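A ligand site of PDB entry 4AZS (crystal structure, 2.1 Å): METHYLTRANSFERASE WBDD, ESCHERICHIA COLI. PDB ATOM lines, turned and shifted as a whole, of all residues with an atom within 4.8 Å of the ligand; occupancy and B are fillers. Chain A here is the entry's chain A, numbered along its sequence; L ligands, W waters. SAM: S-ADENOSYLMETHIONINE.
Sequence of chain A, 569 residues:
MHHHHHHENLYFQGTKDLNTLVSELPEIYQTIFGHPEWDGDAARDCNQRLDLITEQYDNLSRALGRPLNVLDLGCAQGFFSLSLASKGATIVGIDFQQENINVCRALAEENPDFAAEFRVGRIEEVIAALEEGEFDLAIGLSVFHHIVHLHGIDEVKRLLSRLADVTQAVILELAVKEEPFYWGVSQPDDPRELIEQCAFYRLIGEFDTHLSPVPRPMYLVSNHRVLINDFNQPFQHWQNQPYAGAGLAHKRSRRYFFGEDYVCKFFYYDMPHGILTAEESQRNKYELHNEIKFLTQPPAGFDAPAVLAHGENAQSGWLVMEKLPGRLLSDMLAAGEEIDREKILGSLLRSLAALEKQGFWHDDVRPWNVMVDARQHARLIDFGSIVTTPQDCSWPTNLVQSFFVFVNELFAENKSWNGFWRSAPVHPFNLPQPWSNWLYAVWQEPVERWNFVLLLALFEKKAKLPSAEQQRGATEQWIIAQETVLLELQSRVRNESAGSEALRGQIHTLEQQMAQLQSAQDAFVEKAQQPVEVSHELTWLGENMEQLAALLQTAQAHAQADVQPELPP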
ATOM      1  N   TYR A  29      -4.805 -28.097  14.163  1.00  0.00           N
ATOM      2  CA  TYR A  29      -4.583 -27.050  15.121  1.00  0.00           C
ATOM      3  C   TYR A  29      -4.916 -27.586  16.526  1.00  0.00           C
ATOM      4  O   TYR A  29      -4.182 -27.384  17.479  1.00  0.00           O
ATOM      5  CB  TYR A  29      -5.409 -25.808  14.764  1.00  0.00           C
ATOM      6  CG  TYR A  29      -5.096 -24.600  15.573  1.00  0.00           C
ATOM      7  CD1 TYR A  29      -4.020 -23.728  15.226  1.00  0.00           C
ATOM      8  CD2 TYR A  29      -5.818 -24.326  16.714  1.00  0.00           C
ATOM      9  CE1 TYR A  29      -3.711 -22.603  16.022  1.00  0.00           C
ATOM     10  CE2 TYR A  29      -5.533 -23.229  17.518  1.00  0.00           C
ATOM     11  CZ  TYR A  29      -4.482 -22.378  17.195  1.00  0.00           C
ATOM     12  OH  TYR A  29      -4.301 -21.320  18.069  1.00  0.00           O
ATOM     13  N   GLN A  30      -6.041 -28.293  16.621  1.00  0.00           N
ATOM     14  CA  GLN A  30      -6.557 -28.775  17.857  1.00  0.00           C
ATOM     15  C   GLN A  30      -6.500 -30.279  17.916  1.00  0.00           C
ATOM     16  O   GLN A  30      -6.463 -30.952  16.902  1.00  0.00           O
ATOM     17  CB  GLN A  30      -8.044 -28.451  17.974  1.00  0.00           C
ATOM     18  CG  GLN A  30      -8.403 -26.989  17.911  1.00  0.00           C
ATOM     19  CD  GLN A  30      -9.887 -26.793  17.911  1.00  0.00           C
ATOM     20  OE1 GLN A  30     -10.637 -27.626  17.380  1.00  0.00           O
ATOM     21  NE2 GLN A  30     -10.330 -25.685  18.497  1.00  0.00           N
ATOM     22  N   ARG A  44      -2.061 -27.447  19.462  1.00  0.00           N
ATOM     23  CA  ARG A  44      -2.430 -27.125  20.849  1.00  0.00           C
ATOM     24  C   ARG A  44      -3.300 -28.213  21.406  1.00  0.00           C
ATOM     25  O   ARG A  44      -4.247 -28.650  20.759  1.00  0.00           O
ATOM     26  CB  ARG A  44      -3.186 -25.793  20.884  1.00  0.00           C
ATOM     27  CG  ARG A  44      -2.454 -24.701  20.059  1.00  0.00           C
ATOM     28  CD  ARG A  44      -3.022 -23.304  20.249  1.00  0.00           C
ATOM     29  NE  ARG A  44      -2.974 -22.869  21.671  1.00  0.00           N
ATOM     30  CZ  ARG A  44      -3.553 -21.768  22.124  1.00  0.00           C
ATOM     31  NH1 ARG A  44      -4.217 -20.954  21.293  1.00  0.00           N
ATOM     32  NH2 ARG A  44      -3.514 -21.470  23.410  1.00  0.00           N
ATOM     33  N   CYS A  46      -5.332 -28.039  23.973  1.00  0.00           N
ATOM     34  CA  CYS A  46      -6.642 -27.507  24.302  1.00  0.00           C
ATOM     35  C   CYS A  46      -7.164 -27.848  25.687  1.00  0.00           C
ATOM     36  O   CYS A  46      -8.203 -27.314  26.075  1.00  0.00           O
ATOM     37  CB  CYS A  46      -7.697 -27.918  23.276  1.00  0.00           C
ATOM     38  SG  CYS A  46      -7.389 -27.299  21.593  1.00  0.00           S
ATOM     39  N   ARG A  49      -7.267 -24.580  28.127  1.00  0.00           N
ATOM     40  CA  ARG A  49      -8.351 -23.669  27.783  1.00  0.00           C
ATOM     41  C   ARG A  49      -9.691 -24.300  28.071  1.00  0.00           C
ATOM     42  O   ARG A  49     -10.581 -23.648  28.626  1.00  0.00           O
ATOM     43  CB  ARG A  49      -8.229 -23.184  26.315  1.00  0.00           C
ATOM     44  CG  ARG A  49      -7.020 -22.260  26.134  1.00  0.00           C
ATOM     45  CD  ARG A  49      -6.793 -21.804  24.703  1.00  0.00           C
ATOM     46  NE  ARG A  49      -6.683 -22.887  23.758  1.00  0.00           N
ATOM     47  CZ  ARG A  49      -6.968 -22.796  22.470  1.00  0.00           C
ATOM     48  NH1 ARG A  49      -7.408 -21.628  21.936  1.00  0.00           N
ATOM     49  NH2 ARG A  49      -6.801 -23.845  21.693  1.00  0.00           N
ATOM     50  N   LEU A  73     -16.708 -19.396  17.269  1.00  0.00           N
ATOM     51  CA  LEU A  73     -16.256 -18.625  16.132  1.00  0.00           C
ATOM     52  C   LEU A  73     -14.825 -18.996  15.763  1.00  0.00           C
ATOM     53  O   LEU A  73     -13.912 -18.829  16.585  1.00  0.00           O
ATOM     54  CB  LEU A  73     -16.302 -17.125  16.451  1.00  0.00           C
ATOM     55  CG  LEU A  73     -17.742 -16.623  16.612  1.00  0.00           C
ATOM     56  CD1 LEU A  73     -17.739 -15.212  17.170  1.00  0.00           C
ATOM     57  CD2 LEU A  73     -18.493 -16.684  15.322  1.00  0.00           C
ATOM     58  N   GLY A  74     -14.651 -19.474  14.543  1.00  0.00           N
ATOM     59  CA  GLY A  74     -13.386 -20.045  14.118  1.00  0.00           C
ATOM     60  C   GLY A  74     -13.104 -21.338  14.854  1.00  0.00           C
ATOM     61  O   GLY A  74     -12.018 -21.508  15.485  1.00  0.00           O
ATOM     62  N   CYS A  75     -14.055 -22.277  14.719  1.00  0.00           N
ATOM     63  CA  CYS A  75     -14.106 -23.418  15.571  1.00  0.00           C
ATOM     64  C   CYS A  75     -13.080 -24.465  15.205  1.00  0.00           C
ATOM     65  O   CYS A  75     -12.926 -25.452  15.949  1.00  0.00           O
ATOM     66  CB  CYS A  75     -15.509 -24.012  15.562  1.00  0.00           C
ATOM     67  SG  CYS A  75     -16.020 -24.563  13.900  1.00  0.00           S
ATOM     68  N   ALA A  76     -12.424 -24.307  14.045  1.00  0.00           N
ATOM     69  CA  ALA A  76     -11.314 -25.219  13.631  1.00  0.00           C
ATOM     70  C   ALA A  76     -11.782 -26.675  13.584  1.00  0.00           C
ATOM     71  O   ALA A  76     -12.719 -26.959  12.836  1.00  0.00           O
ATOM     72  CB  ALA A  76     -10.095 -25.045  14.521  1.00  0.00           C
ATOM     73  N   PHE A  80     -13.640 -27.491  21.122  1.00  0.00           N
ATOM     74  CA  PHE A  80     -14.404 -26.807  22.179  1.00  0.00           C
ATOM     75  C   PHE A  80     -15.885 -27.018  22.037  1.00  0.00           C
ATOM     76  O   PHE A  80     -16.590 -27.245  23.006  1.00  0.00           O
ATOM     77  CB  PHE A  80     -14.015 -25.328  22.275  1.00  0.00           C
ATOM     78  CG  PHE A  80     -12.577 -25.137  22.638  1.00  0.00           C
ATOM     79  CD1 PHE A  80     -12.184 -25.171  23.962  1.00  0.00           C
ATOM     80  CD2 PHE A  80     -11.613 -25.011  21.668  1.00  0.00           C
ATOM     81  CE1 PHE A  80     -10.876 -25.047  24.309  1.00  0.00           C
ATOM     82  CE2 PHE A  80     -10.275 -24.859  22.014  1.00  0.00           C
ATOM     83  CZ  PHE A  80      -9.895 -24.896  23.337  1.00  0.00           C
ATOM     84  N   ILE A  94     -18.517 -22.166  13.671  1.00  0.00           N
ATOM     85  CA  ILE A  94     -18.319 -21.505  12.413  1.00  0.00           C
ATOM     86  C   ILE A  94     -16.853 -21.491  12.093  1.00  0.00           C
ATOM     87  O   ILE A  94     -16.061 -21.128  12.954  1.00  0.00           O
ATOM     88  CB  ILE A  94     -18.770 -20.028  12.550  1.00  0.00           C
ATOM     89  CG1 ILE A  94     -20.238 -19.948  12.958  1.00  0.00           C
ATOM     90  CG2 ILE A  94     -18.516 -19.251  11.298  1.00  0.00           C
ATOM     91  CD1 ILE A  94     -21.204 -20.564  11.992  1.00  0.00           C
ATOM     92  N   ASP A  95     -16.493 -21.809  10.854  1.00  0.00           N
ATOM     93  CA  ASP A  95     -15.114 -21.652  10.386  1.00  0.00           C
ATOM     94  C   ASP A  95     -15.082 -21.389   8.886  1.00  0.00           C
ATOM     95  O   ASP A  95     -15.924 -21.939   8.191  1.00  0.00           O
ATOM     96  CB  ASP A  95     -14.300 -22.925  10.685  1.00  0.00           C
ATOM     97  CG  ASP A  95     -12.807 -22.682  10.748  1.00  0.00           C
ATOM     98  OD1 ASP A  95     -12.150 -22.721   9.664  1.00  0.00           O
ATOM     99  OD2 ASP A  95     -12.310 -22.429  11.887  1.00  0.00           O
ATOM    100  N   PHE A  96     -14.145 -20.575   8.394  1.00  0.00           N
ATOM    101  CA  PHE A  96     -14.151 -20.321   6.942  1.00  0.00           C
ATOM    102  C   PHE A  96     -13.424 -21.332   6.075  1.00  0.00           C
ATOM    103  O   PHE A  96     -13.406 -21.208   4.832  1.00  0.00           O
ATOM    104  CB  PHE A  96     -13.843 -18.888   6.547  1.00  0.00           C
ATOM    105  CG  PHE A  96     -12.428 -18.426   6.721  1.00  0.00           C
ATOM    106  CD1 PHE A  96     -11.439 -19.200   7.242  1.00  0.00           C
ATOM    107  CD2 PHE A  96     -12.120 -17.135   6.305  1.00  0.00           C
ATOM    108  CE1 PHE A  96     -10.141 -18.722   7.376  1.00  0.00           C
ATOM    109  CE2 PHE A  96     -10.833 -16.637   6.436  1.00  0.00           C
ATOM    110  CZ  PHE A  96      -9.839 -17.437   6.981  1.00  0.00           C
ATOM    111  N   GLN A  97     -12.881 -22.381   6.681  1.00  0.00           N
ATOM    112  CA  GLN A  97     -12.243 -23.448   5.924  1.00  0.00           C
ATOM    113  C   GLN A  97     -13.087 -24.695   5.897  1.00  0.00           C
ATOM    114  O   GLN A  97     -13.410 -25.290   6.945  1.00  0.00           O
ATOM    115  CB  GLN A  97     -10.881 -23.761   6.521  1.00  0.00           C
ATOM    116  CG  GLN A  97      -9.897 -22.638   6.271  1.00  0.00           C
ATOM    117  CD  GLN A  97      -8.512 -23.026   6.720  1.00  0.00           C
ATOM    118  OE1 GLN A  97      -7.861 -23.819   6.057  1.00  0.00           O
ATOM    119  NE2 GLN A  97      -8.066 -22.493   7.875  1.00  0.00           N
ATOM    120  N   ASN A 100     -11.945 -27.819   7.670  1.00  0.00           N
ATOM    121  CA  ASN A 100     -12.153 -27.867   9.084  1.00  0.00           C
ATOM    122  C   ASN A 100     -13.574 -28.278   9.388  1.00  0.00           C
ATOM    123  O   ASN A 100     -13.804 -29.139  10.227  1.00  0.00           O
ATOM    124  CB  ASN A 100     -11.890 -26.511   9.710  1.00  0.00           C
ATOM    125  CG  ASN A 100     -10.419 -26.150   9.743  1.00  0.00           C
ATOM    126  OD1 ASN A 100      -9.534 -27.013   9.712  1.00  0.00           O
ATOM    127  ND2 ASN A 100     -10.149 -24.859   9.946  1.00  0.00           N
ATOM    128  N   GLY A 121     -18.317 -20.376   7.113  1.00  0.00           N
ATOM    129  CA  GLY A 121     -18.698 -18.982   6.918  1.00  0.00           C
ATOM    130  C   GLY A 121     -17.712 -18.097   7.571  1.00  0.00           C
ATOM    131  O   GLY A 121     -16.801 -18.561   8.261  1.00  0.00           O
ATOM    132  N   ARG A 122     -17.855 -16.822   7.296  1.00  0.00           N
ATOM    133  CA  ARG A 122     -16.929 -15.819   7.802  1.00  0.00           C
ATOM    134  C   ARG A 122     -17.509 -15.243   9.082  1.00  0.00           C
ATOM    135  O   ARG A 122     -18.689 -14.895   9.155  1.00  0.00           O
ATOM    136  CB  ARG A 122     -16.699 -14.694   6.780  1.00  0.00           C
ATOM    137  CG  ARG A 122     -15.942 -15.078   5.518  1.00  0.00           C
ATOM    138  CD  ARG A 122     -15.349 -13.857   4.774  1.00  0.00           C
ATOM    139  NE  ARG A 122     -14.312 -13.120   5.566  1.00  0.00           N
ATOM    140  CZ  ARG A 122     -12.987 -13.371   5.524  1.00  0.00           C
ATOM    141  NH1 ARG A 122     -12.518 -14.342   4.738  1.00  0.00           N
ATOM    142  NH2 ARG A 122     -12.129 -12.661   6.265  1.00  0.00           N
ATOM    143  N   ILE A 123     -16.669 -15.111  10.069  1.00  0.00           N
ATOM    144  CA  ILE A 123     -17.059 -14.518  11.360  1.00  0.00           C
ATOM    145  C   ILE A 123     -17.708 -13.134  11.227  1.00  0.00           C
ATOM    146  O   ILE A 123     -18.716 -12.846  11.839  1.00  0.00           O
ATOM    147  CB  ILE A 123     -15.828 -14.432  12.236  1.00  0.00           C
ATOM    148  CG1 ILE A 123     -15.461 -15.851  12.651  1.00  0.00           C
ATOM    149  CG2 ILE A 123     -16.049 -13.593  13.485  1.00  0.00           C
ATOM    150  CD1 ILE A 123     -14.076 -15.876  13.209  1.00  0.00           C
ATOM    151  N   GLU A 124     -17.159 -12.277  10.388  1.00  0.00           N
ATOM    152  CA  GLU A 124     -17.730 -10.938  10.164  1.00  0.00           C
ATOM    153  C   GLU A 124     -19.224 -10.988   9.777  1.00  0.00           C
ATOM    154  O   GLU A 124     -20.028 -10.272  10.362  1.00  0.00           O
ATOM    155  CB  GLU A 124     -16.902 -10.188   9.096  1.00  0.00           C
ATOM    156  CG  GLU A 124     -15.409 -10.084   9.431  1.00  0.00           C
ATOM    157  CD  GLU A 124     -14.503 -11.191   8.817  1.00  0.00           C
ATOM    158  OE1 GLU A 124     -14.904 -12.356   8.716  1.00  0.00           O
ATOM    159  OE2 GLU A 124     -13.345 -10.896   8.455  1.00  0.00           O
ATOM    160  N   LEU A 141     -11.557 -17.808  20.125  1.00  0.00           N
ATOM    161  CA  LEU A 141     -10.229 -18.075  20.632  1.00  0.00           C
ATOM    162  C   LEU A 141      -9.236 -17.983  19.522  1.00  0.00           C
ATOM    163  O   LEU A 141      -9.316 -18.736  18.562  1.00  0.00           O
ATOM    164  CB  LEU A 141     -10.177 -19.481  21.238  1.00  0.00           C
ATOM    165  CG  LEU A 141     -11.319 -19.848  22.136  1.00  0.00           C
ATOM    166  CD1 LEU A 141     -11.142 -21.254  22.677  1.00  0.00           C
ATOM    167  CD2 LEU A 141     -11.500 -18.857  23.269  1.00  0.00           C
ATOM    168  N   SER A 142      -8.261 -17.088  19.646  1.00  0.00           N
ATOM    169  CA  SER A 142      -7.219 -16.955  18.670  1.00  0.00           C
ATOM    170  C   SER A 142      -7.723 -16.809  17.220  1.00  0.00           C
ATOM    171  O   SER A 142      -7.156 -17.328  16.260  1.00  0.00           O
ATOM    172  CB  SER A 142      -6.264 -18.135  18.796  1.00  0.00           C
ATOM    173  OG  SER A 142      -5.513 -18.006  19.978  1.00  0.00           O
ATOM    174  N   VAL A 143      -8.770 -16.011  17.032  1.00  0.00           N
ATOM    175  CA  VAL A 143      -9.261 -15.816  15.695  1.00  0.00           C
ATOM    176  C   VAL A 143      -9.347 -14.332  15.304  1.00  0.00           C
ATOM    177  O   VAL A 143      -9.144 -13.960  14.114  1.00  0.00           O
ATOM    178  CB  VAL A 143     -10.591 -16.591  15.541  1.00  0.00           C
ATOM    179  CG1 VAL A 143     -11.676 -16.043  16.485  1.00  0.00           C
ATOM    180  CG2 VAL A 143     -11.036 -16.491  14.116  1.00  0.00           C
ATOM    181  N   HIS A 146      -6.773 -12.364  13.138  1.00  0.00           N
ATOM    182  CA  HIS A 146      -6.829 -12.505  11.708  1.00  0.00           C
ATOM    183  C   HIS A 146      -7.743 -11.444  11.110  1.00  0.00           C
ATOM    184  O   HIS A 146      -7.513 -11.010   9.993  1.00  0.00           O
ATOM    185  CB  HIS A 146      -7.352 -13.885  11.300  1.00  0.00           C
ATOM    186  CG  HIS A 146      -6.452 -15.035  11.687  1.00  0.00           C
ATOM    187  ND1 HIS A 146      -6.651 -15.799  12.804  1.00  0.00           N
ATOM    188  CD2 HIS A 146      -5.309 -15.591  11.047  1.00  0.00           C
ATOM    189  CE1 HIS A 146      -5.688 -16.754  12.875  1.00  0.00           C
ATOM    190  NE2 HIS A 146      -4.892 -16.629  11.802  1.00  0.00           N
ATOM    191  N   ILE A 147      -8.780 -11.043  11.837  1.00  0.00           N
ATOM    192  CA  ILE A 147      -9.752 -10.045  11.362  1.00  0.00           C
ATOM    193  C   ILE A 147      -9.145  -8.629  11.523  1.00  0.00           C
ATOM    194  O   ILE A 147      -9.332  -7.742  10.682  1.00  0.00           O
ATOM    195  CB  ILE A 147     -11.099 -10.219  12.102  1.00  0.00           C
ATOM    196  CG1 ILE A 147     -11.615 -11.639  11.867  1.00  0.00           C
ATOM    197  CG2 ILE A 147     -12.166  -9.253  11.633  1.00  0.00           C
ATOM    198  CD1 ILE A 147     -12.763 -12.048  12.754  1.00  0.00           C
ATOM    199  N   GLU A 173      -9.734 -15.476  23.639  1.00  0.00           N
ATOM    200  CA  GLU A 173      -8.295 -15.574  23.714  1.00  0.00           C
ATOM    201  C   GLU A 173      -7.753 -14.689  22.620  1.00  0.00           C
ATOM    202  O   GLU A 173      -8.071 -14.886  21.451  1.00  0.00           O
ATOM    203  CB  GLU A 173      -7.817 -16.985  23.499  1.00  0.00           C
ATOM    204  CG  GLU A 173      -6.312 -17.155  23.717  1.00  0.00           C
ATOM    205  CD  GLU A 173      -5.811 -18.529  23.328  1.00  0.00           C
ATOM    206  OE1 GLU A 173      -6.319 -19.074  22.300  1.00  0.00           O
ATOM    207  OE2 GLU A 173      -4.901 -19.032  24.046  1.00  0.00           O
HETATM  208  N   SAM L   1     -10.513 -21.180  17.780  1.00  0.00           N
HETATM  209  CA  SAM L   1      -9.627 -22.326  17.571  1.00  0.00           C
HETATM  210  C   SAM L   1      -8.799 -22.519  18.807  1.00  0.00           C
HETATM  211  O   SAM L   1      -8.388 -21.489  19.391  1.00  0.00           O
HETATM  212  OXT SAM L   1      -8.579 -23.668  19.192  1.00  0.00           O
HETATM  213  CB  SAM L   1      -8.743 -22.138  16.360  1.00  0.00           C
HETATM  214  CG  SAM L   1      -7.820 -20.930  16.269  1.00  0.00           C
HETATM  215  SD  SAM L   1      -7.026 -20.829  14.768  1.00  0.00           S
HETATM  216  CE  SAM L   1      -5.585 -20.058  15.038  1.00  0.00           C
HETATM  217  C5' SAM L   1      -7.977 -19.760  13.889  1.00  0.00           C
HETATM  218  C4' SAM L   1      -9.208 -20.437  13.242  1.00  0.00           C
HETATM  219  O4' SAM L   1     -10.122 -19.475  12.751  1.00  0.00           O
HETATM  220  C3' SAM L   1      -8.854 -21.258  11.990  1.00  0.00           C
HETATM  221  O3' SAM L   1      -9.610 -22.470  12.074  1.00  0.00           O
HETATM  222  C2' SAM L   1      -9.299 -20.461  10.770  1.00  0.00           C
HETATM  223  O2' SAM L   1      -9.837 -21.245   9.706  1.00  0.00           O
HETATM  224  C1' SAM L   1     -10.472 -19.710  11.362  1.00  0.00           C
HETATM  225  N9  SAM L   1     -10.729 -18.369  10.798  1.00  0.00           N
HETATM  226  C8  SAM L   1      -9.828 -17.368  10.678  1.00  0.00           C
HETATM  227  N7  SAM L   1     -10.430 -16.244  10.228  1.00  0.00           N
HETATM  228  C5  SAM L   1     -11.746 -16.547  10.049  1.00  0.00           C
HETATM  229  C6  SAM L   1     -12.925 -15.823   9.609  1.00  0.00           C
HETATM  230  N6  SAM L   1     -12.729 -14.524   9.232  1.00  0.00           N
HETATM  231  N1  SAM L   1     -14.125 -16.457   9.598  1.00  0.00           N
HETATM  232  C2  SAM L   1     -14.230 -17.743   9.957  1.00  0.00           C
HETATM  233  N3  SAM L   1     -13.180 -18.474  10.395  1.00  0.00           N
HETATM  234  C4  SAM L   1     -11.947 -17.936  10.441  1.00  0.00           C
HETATM  235  O   HOH W   1     -12.738 -22.724  19.365  1.00  0.00           O
HETATM  236  O   HOH W   2      -9.078 -13.995   8.381  1.00  0.00           O
HETATM  237  O   HOH W   3      -7.635 -24.642  12.035  1.00  0.00           O
HETATM  238  O   HOH W   4     -13.138 -19.833  18.963  1.00  0.00           O
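NH1 of Arg 49 is in salt-bridge range of O of the ligand (2.7 Å).
NE2 of Gln 97 is in hydrogen-bond range of O2' of the ligand, 2.8 Å away.
N of Ile 123 is in hydrogen-bond range of N1 of the ligand (2.9 Å).
The side-chain carboxylate (OD2) of Asp 95 lies within hydrogen-bond range of an oxygen (O3') of the ligand, 2.7 Å away.
N6 of the ligand lies within hydrogen-bond range of OE1 of Glu 124 (3.1 Å).
N of the ligand sits at hydrogen-bond distance from O of Gly 74, at 2.8 Å.
A nitrogen (N) of the ligand sits at hydrogen-bond distance from the backbone carbonyl oxygen (O) of Leu 141 (2.8 Å).
An oxygen (OXT) of the ligand lies within hydrogen-bond range of the side-chain amide nitrogen of Gln 30 (2.8 Å).
N3 of the ligand lies within hydrogen-bond range of N of Phe 96 (3.1 Å).
The side-chain amide nitrogen (ND2) of Asn 100 lies within hydrogen-bond range of an oxygen (O3') of the ligand (3.2 Å).
OD2 of Asp 95 sits at hydrogen-bond distance from N of Cys 75, at 3.3 Å.
The backbone carbonyl oxygen (O) of Asp 95 lies within hydrogen-bond range of the backbone NH (N) of Gly 121, at 3.1 Å.
The backbone NH of Gln 97 is in hydrogen-bond range of the side-chain carboxylate of Asp 95, 3.1 Å away.
The guanidinium group of Arg 122 is in salt-bridge range of the side-chain carboxylate of Glu 124 (3.1 Å).
N of Phe 96 is in hydrogen-bond range of O of Gly 121 (3.3 Å).
OE1 of Gln 30 lies close to O of Cys 75 (3.5 Å).
The backbone carbonyl oxygen (O) of Tyr 29 sits at hydrogen-bond distance from the backbone NH (N) of Arg 44, at 2.9 Å.
OD1 of Asp 95 lies within hydrogen-bond range of ND2 of Asn 100, at 2.9 Å.
Tyr 29 touches the ligand.
Ala 76 touches the ligand.
Phe 80 touches the ligand (CE2 to OXT, 3.5 Å).
Gly 121 touches the ligand.
Arg 122 touches the ligand.
Ser 142 touches the ligand.
Val 143 touches the ligand (CG2 to O4', 3.4 Å).
His 146 touches the ligand (CE1 to C5', 3.9 Å).
Hydrophobic or aromatic side chains that line the ligand: Tyr 29, Ala 76, Phe 80, Phe 96, Ile 123, Leu 141, Val 143 and His 146.
Water W3 lies within hydrogen-bond range of an oxygen (O3') of the ligand and the side-chain amide nitrogen of Asn 100.
Water W4 lies within hydrogen-bond range of O of Leu 73, N of Leu 141 and N of the ligand.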
